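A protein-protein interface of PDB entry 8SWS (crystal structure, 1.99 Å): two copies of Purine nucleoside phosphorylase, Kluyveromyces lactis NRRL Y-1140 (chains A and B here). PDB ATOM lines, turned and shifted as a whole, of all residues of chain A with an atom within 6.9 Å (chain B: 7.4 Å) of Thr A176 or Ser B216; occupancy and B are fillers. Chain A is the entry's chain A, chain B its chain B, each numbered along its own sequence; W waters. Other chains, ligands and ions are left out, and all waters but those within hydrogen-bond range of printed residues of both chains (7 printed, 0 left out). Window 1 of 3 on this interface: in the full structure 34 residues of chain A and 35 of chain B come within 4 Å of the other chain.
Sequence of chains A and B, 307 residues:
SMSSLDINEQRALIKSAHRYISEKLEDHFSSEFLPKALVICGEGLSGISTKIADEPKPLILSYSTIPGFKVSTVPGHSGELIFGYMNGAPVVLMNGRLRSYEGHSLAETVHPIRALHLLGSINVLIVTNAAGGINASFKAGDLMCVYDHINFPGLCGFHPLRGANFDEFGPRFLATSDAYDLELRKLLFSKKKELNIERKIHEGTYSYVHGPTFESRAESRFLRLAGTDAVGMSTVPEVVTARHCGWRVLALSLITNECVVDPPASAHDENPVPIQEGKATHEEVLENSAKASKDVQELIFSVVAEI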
ATOM      1  N   TYR A 147      19.089  36.802   9.376  1.00  0.00           N
ATOM      2  CA  TYR A 147      19.849  36.837   8.130  1.00  0.00           C
ATOM      3  C   TYR A 147      20.167  35.415   7.708  1.00  0.00           C
ATOM      4  O   TYR A 147      20.693  35.208   6.619  1.00  0.00           O
ATOM      5  CB  TYR A 147      21.076  37.741   8.362  1.00  0.00           C
ATOM      6  CG  TYR A 147      22.328  37.166   8.953  1.00  0.00           C
ATOM      7  CD1 TYR A 147      22.310  36.298  10.033  1.00  0.00           C
ATOM      8  CD2 TYR A 147      23.500  37.941   8.826  1.00  0.00           C
ATOM      9  CE1 TYR A 147      23.489  35.862  10.646  1.00  0.00           C
ATOM     10  CE2 TYR A 147      24.704  37.604   9.508  1.00  0.00           C
ATOM     11  CZ  TYR A 147      24.689  36.588  10.423  1.00  0.00           C
ATOM     12  OH  TYR A 147      25.858  36.248  11.051  1.00  0.00           O
ATOM     13  N   ASP A 148      19.750  34.423   8.509  1.00  0.00           N
ATOM     14  CA  ASP A 148      19.945  33.005   8.205  1.00  0.00           C
ATOM     15  C   ASP A 148      19.011  32.187   9.108  1.00  0.00           C
ATOM     16  O   ASP A 148      18.522  32.685  10.136  1.00  0.00           O
ATOM     17  CB  ASP A 148      21.386  32.592   8.469  1.00  0.00           C
ATOM     18  CG  ASP A 148      21.778  31.324   7.734  1.00  0.00           C
ATOM     19  OD1 ASP A 148      20.971  30.782   6.957  1.00  0.00           O
ATOM     20  OD2 ASP A 148      22.884  30.840   7.983  1.00  0.00           O
ATOM     21  N   HIS A 149      18.805  30.918   8.763  1.00  0.00           N
ATOM     22  CA  HIS A 149      18.031  30.096   9.683  1.00  0.00           C
ATOM     23  C   HIS A 149      18.541  28.665   9.757  1.00  0.00           C
ATOM     24  O   HIS A 149      19.374  28.221   8.966  1.00  0.00           O
ATOM     25  CB  HIS A 149      16.529  30.034   9.358  1.00  0.00           C
ATOM     26  CG  HIS A 149      16.196  29.434   8.030  1.00  0.00           C
ATOM     27  ND1 HIS A 149      15.420  30.094   7.101  1.00  0.00           N
ATOM     28  CD2 HIS A 149      16.553  28.251   7.463  1.00  0.00           C
ATOM     29  CE1 HIS A 149      15.283  29.324   6.034  1.00  0.00           C
ATOM     30  NE2 HIS A 149      15.975  28.212   6.220  1.00  0.00           N
ATOM     31  N   ILE A 150      17.997  27.928  10.722  1.00  0.00           N
ATOM     32  CA  ILE A 150      18.251  26.500  10.849  1.00  0.00           C
ATOM     33  C   ILE A 150      16.891  25.821  10.872  1.00  0.00           C
ATOM     34  O   ILE A 150      16.063  26.128  11.735  1.00  0.00           O
ATOM     35  CB  ILE A 150      19.074  26.149  12.101  1.00  0.00           C
ATOM     36  CG1 ILE A 150      20.473  26.829  12.064  1.00  0.00           C
ATOM     37  CG2 ILE A 150      19.212  24.588  12.263  1.00  0.00           C
ATOM     38  CD1 ILE A 150      21.358  26.430  13.258  1.00  0.00           C
ATOM     39  N   ASN A 151      16.653  24.961   9.876  1.00  0.00           N
ATOM     40  CA  ASN A 151      15.444  24.134   9.763  1.00  0.00           C
ATOM     41  C   ASN A 151      15.742  22.689  10.123  1.00  0.00           C
ATOM     42  O   ASN A 151      15.705  21.803   9.288  1.00  0.00           O
ATOM     43  CB  ASN A 151      14.834  24.258   8.379  1.00  0.00           C
ATOM     44  CG  ASN A 151      13.398  23.740   8.314  1.00  0.00           C
ATOM     45  OD1 ASN A 151      12.759  23.446   9.330  1.00  0.00           O
ATOM     46  ND2 ASN A 151      12.846  23.764   7.112  1.00  0.00           N
ATOM     47  N   HIS A 159       8.841  19.101   6.555  1.00  0.00           N
ATOM     48  CA  HIS A 159       9.320  20.110   5.615  1.00  0.00           C
ATOM     49  C   HIS A 159       8.134  20.610   4.803  1.00  0.00           C
ATOM     50  O   HIS A 159       7.354  19.793   4.299  1.00  0.00           O
ATOM     51  CB  HIS A 159      10.393  19.491   4.704  1.00  0.00           C
ATOM     52  CG  HIS A 159      11.206  20.504   3.965  1.00  0.00           C
ATOM     53  ND1 HIS A 159      10.641  21.393   3.068  1.00  0.00           N
ATOM     54  CD2 HIS A 159      12.531  20.782   3.994  1.00  0.00           C
ATOM     55  CE1 HIS A 159      11.590  22.190   2.586  1.00  0.00           C
ATOM     56  NE2 HIS A 159      12.744  21.839   3.133  1.00  0.00           N
ATOM     57  N   LEU A 174      15.266  23.954  -3.985  1.00  0.00           N
ATOM     58  CA  LEU A 174      15.367  25.358  -3.613  1.00  0.00           C
ATOM     59  C   LEU A 174      16.581  25.598  -2.735  1.00  0.00           C
ATOM     60  O   LEU A 174      16.680  25.002  -1.659  1.00  0.00           O
ATOM     61  CB  LEU A 174      14.108  25.774  -2.858  1.00  0.00           C
ATOM     62  CG  LEU A 174      14.031  27.241  -2.449  1.00  0.00           C
ATOM     63  CD1 LEU A 174      13.934  28.162  -3.689  1.00  0.00           C
ATOM     64  CD2 LEU A 174      12.827  27.422  -1.511  1.00  0.00           C
ATOM     65  N   ALA A 175      17.466  26.512  -3.148  1.00  0.00           N
ATOM     66  CA  ALA A 175      18.551  26.929  -2.264  1.00  0.00           C
ATOM     67  C   ALA A 175      18.010  27.792  -1.136  1.00  0.00           C
ATOM     68  O   ALA A 175      16.989  28.467  -1.283  1.00  0.00           O
ATOM     69  CB  ALA A 175      19.622  27.710  -3.048  1.00  0.00           C
ATOM     70  N   THR A 176      18.684  27.749   0.021  1.00  0.00           N
ATOM     71  CA  THR A 176      18.324  28.639   1.117  1.00  0.00           C
ATOM     72  C   THR A 176      19.528  29.392   1.663  1.00  0.00           C
ATOM     73  O   THR A 176      19.377  30.129   2.650  1.00  0.00           O
ATOM     74  CB  THR A 176      17.612  27.901   2.286  1.00  0.00           C
ATOM     75  OG1 THR A 176      18.437  26.850   2.806  1.00  0.00           O
ATOM     76  CG2 THR A 176      16.271  27.265   1.804  1.00  0.00           C
ATOM     77  N   SER A 177      20.703  29.277   1.023  1.00  0.00           N
ATOM     78  CA  SER A 177      21.843  30.126   1.374  1.00  0.00           C
ATOM     79  C   SER A 177      21.642  31.595   0.977  1.00  0.00           C
ATOM     80  O   SER A 177      22.434  32.460   1.400  1.00  0.00           O
ATOM     81  CB  SER A 177      23.112  29.523   0.757  1.00  0.00           C
ATOM     82  OG  SER A 177      23.065  29.475  -0.685  1.00  0.00           O
ATOM     83  N   ASP A 178      20.596  31.903   0.201  1.00  0.00           N
ATOM     84  CA  ASP A 178      20.246  33.273  -0.191  1.00  0.00           C
ATOM     85  C   ASP A 178      18.843  33.633   0.275  1.00  0.00           C
ATOM     86  O   ASP A 178      18.095  34.330  -0.426  1.00  0.00           O
ATOM     87  CB  ASP A 178      20.328  33.457  -1.708  1.00  0.00           C
ATOM     88  CG  ASP A 178      19.399  32.490  -2.463  1.00  0.00           C
ATOM     89  OD1 ASP A 178      18.931  31.491  -1.862  1.00  0.00           O
ATOM     90  OD2 ASP A 178      19.120  32.758  -3.642  1.00  0.00           O
ATOM     91  N   ALA A 179      18.445  33.145   1.444  1.00  0.00           N
ATOM     92  CA  ALA A 179      17.035  33.292   1.816  1.00  0.00           C
ATOM     93  C   ALA A 179      16.677  34.709   2.276  1.00  0.00           C
ATOM     94  O   ALA A 179      15.524  35.144   2.090  1.00  0.00           O
ATOM     95  CB  ALA A 179      16.669  32.274   2.913  1.00  0.00           C
ATOM     96  N   TYR A 180      17.612  35.443   2.880  1.00  0.00           N
ATOM     97  CA  TYR A 180      17.282  36.698   3.591  1.00  0.00           C
ATOM     98  C   TYR A 180      17.955  37.882   2.886  1.00  0.00           C
ATOM     99  O   TYR A 180      19.092  38.217   3.189  1.00  0.00           O
ATOM    100  CB  TYR A 180      17.720  36.582   5.062  1.00  0.00           C
ATOM    101  CG  TYR A 180      16.903  35.516   5.772  1.00  0.00           C
ATOM    102  CD1 TYR A 180      15.584  35.782   6.203  1.00  0.00           C
ATOM    103  CD2 TYR A 180      17.405  34.226   5.923  1.00  0.00           C
ATOM    104  CE1 TYR A 180      14.809  34.805   6.791  1.00  0.00           C
ATOM    105  CE2 TYR A 180      16.600  33.201   6.558  1.00  0.00           C
ATOM    106  CZ  TYR A 180      15.334  33.520   6.986  1.00  0.00           C
ATOM    107  OH  TYR A 180      14.544  32.583   7.578  1.00  0.00           O
ATOM    108  N   THR A 205      20.844  34.184  13.461  1.00  0.00           N
ATOM    109  CA  THR A 205      20.292  32.968  12.899  1.00  0.00           C
ATOM    110  C   THR A 205      19.110  32.558  13.760  1.00  0.00           C
ATOM    111  O   THR A 205      19.252  32.394  14.983  1.00  0.00           O
ATOM    112  CB  THR A 205      21.343  31.859  12.844  1.00  0.00           C
ATOM    113  OG1 THR A 205      22.355  32.234  11.910  1.00  0.00           O
ATOM    114  CG2 THR A 205      20.716  30.501  12.353  1.00  0.00           C
ATOM    115  N   VAL A 239       8.991  31.298   5.368  1.00  0.00           N
ATOM    116  CA  VAL A 239      10.097  31.853   4.573  1.00  0.00           C
ATOM    117  C   VAL A 239      10.402  30.931   3.394  1.00  0.00           C
ATOM    118  O   VAL A 239      10.526  31.375   2.239  1.00  0.00           O
ATOM    119  CB  VAL A 239      11.349  32.066   5.454  1.00  0.00           C
ATOM    120  CG1 VAL A 239      12.643  32.370   4.555  1.00  0.00           C
ATOM    121  CG2 VAL A 239      11.119  33.193   6.471  1.00  0.00           C
ATOM    122  N   VAL A 240      10.500  29.621   3.670  1.00  0.00           N
ATOM    123  CA  VAL A 240      10.849  28.652   2.637  1.00  0.00           C
ATOM    124  C   VAL A 240       9.827  28.705   1.510  1.00  0.00           C
ATOM    125  O   VAL A 240      10.180  28.767   0.317  1.00  0.00           O
ATOM    126  CB  VAL A 240      10.963  27.235   3.252  1.00  0.00           C
ATOM    127  CG1 VAL A 240      11.022  26.125   2.157  1.00  0.00           C
ATOM    128  CG2 VAL A 240      12.198  27.152   4.141  1.00  0.00           C
ATOM    129  N   ARG A 243      10.089  31.869  -0.431  1.00  0.00           N
ATOM    130  CA  ARG A 243      11.226  31.779  -1.349  1.00  0.00           C
ATOM    131  C   ARG A 243      10.904  30.876  -2.536  1.00  0.00           C
ATOM    132  O   ARG A 243      11.314  31.162  -3.675  1.00  0.00           O
ATOM    133  CB  ARG A 243      12.479  31.293  -0.606  1.00  0.00           C
ATOM    134  CG  ARG A 243      13.072  32.317   0.386  1.00  0.00           C
ATOM    135  CD  ARG A 243      13.539  33.588  -0.369  1.00  0.00           C
ATOM    136  NE  ARG A 243      14.591  33.251  -1.324  1.00  0.00           N
ATOM    137  CZ  ARG A 243      14.746  33.835  -2.505  1.00  0.00           C
ATOM    138  NH1 ARG A 243      13.953  34.823  -2.908  1.00  0.00           N
ATOM    139  NH2 ARG A 243      15.759  33.463  -3.282  1.00  0.00           N
ATOM    140  N   ILE B 134      30.575  18.905   2.535  1.00  0.00           N
ATOM    141  CA  ILE B 134      30.530  19.571   3.824  1.00  0.00           C
ATOM    142  C   ILE B 134      31.917  19.689   4.431  1.00  0.00           C
ATOM    143  O   ILE B 134      32.257  20.723   5.008  1.00  0.00           O
ATOM    144  CB  ILE B 134      29.578  18.826   4.795  1.00  0.00           C
ATOM    145  CG1 ILE B 134      28.101  18.910   4.359  1.00  0.00           C
ATOM    146  CG2 ILE B 134      29.719  19.401   6.212  1.00  0.00           C
ATOM    147  CD1 ILE B 134      27.442  20.312   4.610  1.00  0.00           C
ATOM    148  N   THR B 213      15.087  21.242   0.046  1.00  0.00           N
ATOM    149  CA  THR B 213      15.930  22.445   0.000  1.00  0.00           C
ATOM    150  C   THR B 213      17.401  22.085   0.080  1.00  0.00           C
ATOM    151  O   THR B 213      17.800  21.124   0.759  1.00  0.00           O
ATOM    152  CB  THR B 213      15.623  23.426   1.154  1.00  0.00           C
ATOM    153  OG1 THR B 213      15.521  22.713   2.408  1.00  0.00           O
ATOM    154  CG2 THR B 213      14.317  24.203   0.880  1.00  0.00           C
ATOM    155  N   PHE B 214      18.232  22.898  -0.582  1.00  0.00           N
ATOM    156  CA  PHE B 214      19.652  22.858  -0.243  1.00  0.00           C
ATOM    157  C   PHE B 214      19.882  23.581   1.094  1.00  0.00           C
ATOM    158  O   PHE B 214      19.060  24.382   1.539  1.00  0.00           O
ATOM    159  CB  PHE B 214      20.516  23.488  -1.362  1.00  0.00           C
ATOM    160  CG  PHE B 214      20.442  22.778  -2.688  1.00  0.00           C
ATOM    161  CD1 PHE B 214      21.109  21.540  -2.872  1.00  0.00           C
ATOM    162  CD2 PHE B 214      19.749  23.349  -3.764  1.00  0.00           C
ATOM    163  CE1 PHE B 214      21.054  20.873  -4.115  1.00  0.00           C
ATOM    164  CE2 PHE B 214      19.702  22.712  -5.009  1.00  0.00           C
ATOM    165  CZ  PHE B 214      20.342  21.463  -5.183  1.00  0.00           C
ATOM    166  N   GLU B 215      21.016  23.311   1.725  1.00  0.00           N
ATOM    167  CA  GLU B 215      21.220  23.715   3.104  1.00  0.00           C
ATOM    168  C   GLU B 215      21.452  25.226   3.184  1.00  0.00           C
ATOM    169  O   GLU B 215      22.079  25.832   2.298  1.00  0.00           O
ATOM    170  CB  GLU B 215      22.446  23.023   3.712  1.00  0.00           C
ATOM    171  CG  GLU B 215      22.268  21.518   4.086  1.00  0.00           C
ATOM    172  CD  GLU B 215      22.046  20.627   2.846  1.00  0.00           C
ATOM    173  OE1 GLU B 215      22.505  20.968   1.696  1.00  0.00           O
ATOM    174  OE2 GLU B 215      21.286  19.628   2.994  1.00  0.00           O
ATOM    175  N   SER B 216      20.928  25.826   4.249  1.00  0.00           N
ATOM    176  CA  SER B 216      21.337  27.172   4.611  1.00  0.00           C
ATOM    177  C   SER B 216      22.792  27.161   5.081  1.00  0.00           C
ATOM    178  O   SER B 216      23.404  26.106   5.302  1.00  0.00           O
ATOM    179  CB  SER B 216      20.427  27.727   5.722  1.00  0.00           C
ATOM    180  OG  SER B 216      20.764  27.131   6.987  1.00  0.00           O
ATOM    181  N   ARG B 217      23.352  28.359   5.263  1.00  0.00           N
ATOM    182  CA  ARG B 217      24.742  28.438   5.694  1.00  0.00           C
ATOM    183  C   ARG B 217      24.882  27.821   7.071  1.00  0.00           C
ATOM    184  O   ARG B 217      25.783  27.006   7.310  1.00  0.00           O
ATOM    185  CB  ARG B 217      25.224  29.909   5.713  1.00  0.00           C
ATOM    186  CG  ARG B 217      25.182  30.546   4.349  1.00  0.00           C
ATOM    187  CD  ARG B 217      24.829  32.045   4.411  1.00  0.00           C
ATOM    188  NE  ARG B 217      24.660  32.567   3.059  1.00  0.00           N
ATOM    189  CZ  ARG B 217      25.665  32.949   2.276  1.00  0.00           C
ATOM    190  NH1 ARG B 217      26.915  32.882   2.684  1.00  0.00           N
ATOM    191  NH2 ARG B 217      25.409  33.351   1.033  1.00  0.00           N
ATOM    192  N   ALA B 218      23.982  28.205   7.991  1.00  0.00           N
ATOM    193  CA  ALA B 218      24.056  27.688   9.351  1.00  0.00           C
ATOM    194  C   ALA B 218      23.809  26.188   9.381  1.00  0.00           C
ATOM    195  O   ALA B 218      24.461  25.462  10.152  1.00  0.00           O
ATOM    196  CB  ALA B 218      23.057  28.415  10.267  1.00  0.00           C
ATOM    197  N   GLU B 219      22.876  25.712   8.551  1.00  0.00           N
ATOM    198  CA  GLU B 219      22.626  24.271   8.445  1.00  0.00           C
ATOM    199  C   GLU B 219      23.898  23.522   8.036  1.00  0.00           C
ATOM    200  O   GLU B 219      24.230  22.475   8.605  1.00  0.00           O
ATOM    201  CB  GLU B 219      21.504  24.022   7.449  1.00  0.00           C
ATOM    202  CG  GLU B 219      20.093  24.202   8.066  1.00  0.00           C
ATOM    203  CD  GLU B 219      18.980  24.356   7.017  1.00  0.00           C
ATOM    204  OE1 GLU B 219      19.239  24.069   5.812  1.00  0.00           O
ATOM    205  OE2 GLU B 219      17.852  24.749   7.398  1.00  0.00           O
ATOM    206  N   SER B 220      24.626  24.029   7.027  1.00  0.00           N
ATOM    207  CA  SER B 220      25.843  23.328   6.607  1.00  0.00           C
ATOM    208  C   SER B 220      26.927  23.388   7.679  1.00  0.00           C
ATOM    209  O   SER B 220      27.668  22.416   7.876  1.00  0.00           O
ATOM    210  CB  SER B 220      26.366  23.903   5.290  1.00  0.00           C
ATOM    211  OG  SER B 220      25.468  23.631   4.234  1.00  0.00           O
ATOM    212  N   ARG B 221      27.058  24.515   8.368  1.00  0.00           N
ATOM    213  CA  ARG B 221      28.029  24.559   9.460  1.00  0.00           C
ATOM    214  C   ARG B 221      27.628  23.595  10.567  1.00  0.00           C
ATOM    215  O   ARG B 221      28.478  22.913  11.141  1.00  0.00           O
ATOM    216  CB  ARG B 221      28.193  25.980  10.019  1.00  0.00           C
ATOM    217  CG  ARG B 221      28.854  26.957   9.042  1.00  0.00           C
ATOM    218  CD  ARG B 221      29.362  28.247   9.749  1.00  0.00           C
ATOM    219  NE  ARG B 221      28.275  28.801  10.565  1.00  0.00           N
ATOM    220  CZ  ARG B 221      27.352  29.628  10.105  1.00  0.00           C
ATOM    221  NH1 ARG B 221      27.311  29.969   8.822  1.00  0.00           N
ATOM    222  NH2 ARG B 221      26.461  30.142  10.947  1.00  0.00           N
ATOM    223  N   PHE B 222      26.334  23.544  10.893  1.00  0.00           N
ATOM    224  CA  PHE B 222      25.849  22.526  11.827  1.00  0.00           C
ATOM    225  C   PHE B 222      26.246  21.116  11.368  1.00  0.00           C
ATOM    226  O   PHE B 222      26.857  20.348  12.127  1.00  0.00           O
ATOM    227  CB  PHE B 222      24.331  22.618  11.952  1.00  0.00           C
ATOM    228  CG  PHE B 222      23.712  21.385  12.555  1.00  0.00           C
ATOM    229  CD1 PHE B 222      24.003  21.016  13.875  1.00  0.00           C
ATOM    230  CD2 PHE B 222      22.903  20.565  11.785  1.00  0.00           C
ATOM    231  CE1 PHE B 222      23.442  19.859  14.426  1.00  0.00           C
ATOM    232  CE2 PHE B 222      22.355  19.385  12.331  1.00  0.00           C
ATOM    233  CZ  PHE B 222      22.616  19.049  13.653  1.00  0.00           C
ATOM    234  N   LEU B 223      25.892  20.750  10.131  1.00  0.00           N
ATOM    235  CA  LEU B 223      26.266  19.426   9.641  1.00  0.00           C
ATOM    236  C   LEU B 223      27.762  19.184   9.764  1.00  0.00           C
ATOM    237  O   LEU B 223      28.193  18.084  10.128  1.00  0.00           O
ATOM    238  CB  LEU B 223      25.817  19.241   8.190  1.00  0.00           C
ATOM    239  CG  LEU B 223      24.296  19.188   8.067  1.00  0.00           C
ATOM    240  CD1 LEU B 223      23.940  19.303   6.571  1.00  0.00           C
ATOM    241  CD2 LEU B 223      23.713  17.853   8.647  1.00  0.00           C
ATOM    242  N   CYS B 259      29.178  22.939  -0.250  1.00  0.00           N
ATOM    243  CA  CYS B 259      28.118  23.591   0.516  1.00  0.00           C
ATOM    244  C   CYS B 259      28.563  24.947   1.042  1.00  0.00           C
ATOM    245  O   CYS B 259      29.644  25.082   1.619  1.00  0.00           O
ATOM    246  CB  CYS B 259      27.683  22.716   1.684  1.00  0.00           C
ATOM    247  SG  CYS B 259      26.999  21.134   1.097  1.00  0.00           S
ATOM    248  N   VAL B 260      27.696  25.940   0.878  1.00  0.00           N
ATOM    249  CA  VAL B 260      27.974  27.292   1.366  1.00  0.00           C
ATOM    250  C   VAL B 260      27.872  27.296   2.890  1.00  0.00           C
ATOM    251  O   VAL B 260      26.809  26.979   3.451  1.00  0.00           O
ATOM    252  CB  VAL B 260      26.990  28.289   0.743  1.00  0.00           C
ATOM    253  CG1 VAL B 260      27.187  29.736   1.292  1.00  0.00           C
ATOM    254  CG2 VAL B 260      27.077  28.206  -0.784  1.00  0.00           C
ATOM    255  N   VAL B 261      28.984  27.632   3.564  1.00  0.00           N
ATOM    256  CA  VAL B 261      29.033  27.701   5.023  1.00  0.00           C
ATOM    257  C   VAL B 261      29.265  29.112   5.563  1.00  0.00           C
ATOM    258  O   VAL B 261      29.022  29.336   6.758  1.00  0.00           O
ATOM    259  CB  VAL B 261      30.095  26.747   5.626  1.00  0.00           C
ATOM    260  CG1 VAL B 261      29.746  25.292   5.428  1.00  0.00           C
ATOM    261  CG2 VAL B 261      31.559  27.038   5.027  1.00  0.00           C
ATOM    262  N   ASP B 262      29.807  30.038   4.760  1.00  0.00           N
ATOM    263  CA  ASP B 262      30.148  31.344   5.290  1.00  0.00           C
ATOM    264  C   ASP B 262      28.893  32.078   5.763  1.00  0.00           C
ATOM    265  O   ASP B 262      27.848  32.015   5.110  1.00  0.00           O
ATOM    266  CB  ASP B 262      30.850  32.206   4.229  1.00  0.00           C
ATOM    267  CG  ASP B 262      32.292  31.767   3.957  1.00  0.00           C
ATOM    268  OD1 ASP B 262      32.866  31.001   4.771  1.00  0.00           O
ATOM    269  OD2 ASP B 262      32.848  32.242   2.933  1.00  0.00           O
ATOM    270  N   ILE B 275      24.616  37.463  -1.453  1.00  0.00           N
ATOM    271  CA  ILE B 275      24.183  36.254  -0.769  1.00  0.00           C
ATOM    272  C   ILE B 275      23.906  35.132  -1.753  1.00  0.00           C
ATOM    273  O   ILE B 275      23.915  33.961  -1.357  1.00  0.00           O
ATOM    274  CB  ILE B 275      22.942  36.474   0.119  1.00  0.00           C
ATOM    275  CG1 ILE B 275      21.752  36.941  -0.716  1.00  0.00           C
ATOM    276  CG2 ILE B 275      23.250  37.510   1.240  1.00  0.00           C
ATOM    277  CD1 ILE B 275      20.509  37.151   0.136  1.00  0.00           C
ATOM    278  N   LYS B 279      25.583  29.732  -4.751  1.00  0.00           N
ATOM    279  CA  LYS B 279      24.443  28.941  -4.293  1.00  0.00           C
ATOM    280  C   LYS B 279      24.300  27.658  -5.095  1.00  0.00           C
ATOM    281  O   LYS B 279      24.678  27.576  -6.269  1.00  0.00           O
ATOM    282  CB  LYS B 279      23.126  29.697  -4.357  1.00  0.00           C
ATOM    283  CG  LYS B 279      22.584  30.091  -5.721  1.00  0.00           C
ATOM    284  CD  LYS B 279      21.295  30.881  -5.395  1.00  0.00           C
ATOM    285  CE  LYS B 279      20.086  30.506  -6.216  1.00  0.00           C
ATOM    286  NZ  LYS B 279      20.206  31.131  -7.569  1.00  0.00           N
ATOM    287  N   ALA B 280      23.751  26.653  -4.426  1.00  0.00           N
ATOM    288  CA  ALA B 280      23.528  25.352  -5.047  1.00  0.00           C
ATOM    289  C   ALA B 280      22.394  25.452  -6.043  1.00  0.00           C
ATOM    290  O   ALA B 280      21.418  26.179  -5.820  1.00  0.00           O
ATOM    291  CB  ALA B 280      23.194  24.289  -3.979  1.00  0.00           C
HETATM  292  O   HOH W   1      14.506  24.244   4.849  1.00  0.00           O
HETATM  293  O   HOH W   2      24.932  31.946   9.190  1.00  0.00           O
HETATM  294  O   HOH W   3      21.342  30.953   4.558  1.00  0.00           O
HETATM  295  O   HOH W   4      16.895  25.699   5.080  1.00  0.00           O
HETATM  296  O   HOH W   5      24.620  31.413  -1.759  1.00  0.00           O
HETATM  297  O   HOH W   6      21.244  26.455   0.024  1.00  0.00           O
HETATM  298  O   HOH W   7      23.464  26.929  -1.475  1.00  0.00           O
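O of His A149 lies within hydrogen-bond range of OG of Ser B216. O of Leu A174 is in hydrogen-bond range of N of Phe B214 (2.8 Å). The backbone carbonyl oxygen (O) of Ser A177 is in hydrogen-bond range of the guanidinium group (NE) of Arg B217 (2.8 Å). The backbone carbonyl oxygen (O) of Ile B275 sits close to the backbone carbonyl oxygen (O) of Ser A177 (3.5 Å). OG1 of Thr A176 lies within hydrogen-bond range of O of Phe B214 (2.8 Å). N of Ala B218 sits at hydrogen-bond distance from OD2 of Asp A148 (2.9 Å). N of Asn A151 lies within hydrogen-bond range of OE2 of Glu B219 (2.8 Å). N of Ser B216 sits at hydrogen-bond distance from OG1 of Thr A176. The side-chain hydroxyl (OG1) of Thr B213 is in hydrogen-bond range of a ring nitrogen (NE2) of His A159, at 3.0 Å.
OH of Tyr A180 is in hydrogen-bond range of ND1 of His A149. The side-chain carboxylate of Asp A178 is in salt-bridge range of the guanidinium group of Arg A243 (3.5 Å). The side-chain carboxylate (OE1) of Glu B219 is in hydrogen-bond range of the backbone NH (N) of Ser B216. O of Ser B216 lies within hydrogen-bond range of OG of Ser B220, 3.4 Å away.
Asp A148 touches Ser B216 (OD1 to CB, 3.3 Å). OD2 of Asp A148 touches CB of Arg B217, 3.4 Å away. Glu B219 touches Ile A150. Leu A174 touches Thr B213. Ala A175 touches Phe B214. CG2 of Thr A176 touches CG2 of Thr B213, 3.7 Å away. Ser A177 touches Glu B215 (N to O, 3.9 Å). Lys B279 touches Ser A177. OD2 of Asp A178 touches CD of Lys B279, 3.4 Å away. CG2 of Thr A205 touches CB of Ala B218 (3.8 Å).
Of the printed residues of chain B, Ala A175 touches Phe B214 and Ala B280. Of chain B, only Thr B213, Phe B214, Glu B215 and Ser B216 come within 4 Å of Thr A176. Of the printed residues of chain B, Thr A205 touches Ala B218 (3.8 Å). Ser B216 touches three residues of chain A. Of the printed residues of chain A, Arg B217 touches Asp A148 (3.4 Å) and Ser A177 (2.8 Å). Of the printed residues of chain A, Lys B279 touches Ser A177 and Asp A178. The nearest printed residue of chain A that does not touch Ala B218 is Ser A177 (7.2 Å).
Of the 17 printed residues of chain A, 12 touch a printed residue of chain B. Printed residues of chain A that touch a printed residue of chain B: Asp A148, His A149, Ile A150, Asn A151, His A159, Leu A174, Ala A175, Thr A176, Ser A177, Asp A178, Tyr A180 and Thr A205. Hydrophobic or aromatic side chains of chain A within 4 Å of the printed part of chain B: His A149, Ile A150, His A159 and Ala A175. Of the 19 printed residues of chain B, 10 touch a printed residue of chain A. Hydrophobic or aromatic side chains of chain B that line the printed part of chain A: Phe B214, Ala B218 and Ile B275. Among the printed residues, no Asp or Glu carboxylate lies within 4 Å of a Lys or Arg side-chain nitrogen of the other chain.
No position is printed for both chains. Of the 26 pairs that touch across the chains among the printed residues, none has its exchanged pair printed and touching as well.
Water W3 lies within hydrogen-bond range of the side-chain carboxylate (OD1) of Asp A148, the backbone carbonyl oxygen (O) of Thr A176 and the backbone NH (N) of Arg B217. Water W4 lies within hydrogen-bond range of OE2 of Glu B219, NE2 of His A149 and OG1 of Thr A176.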
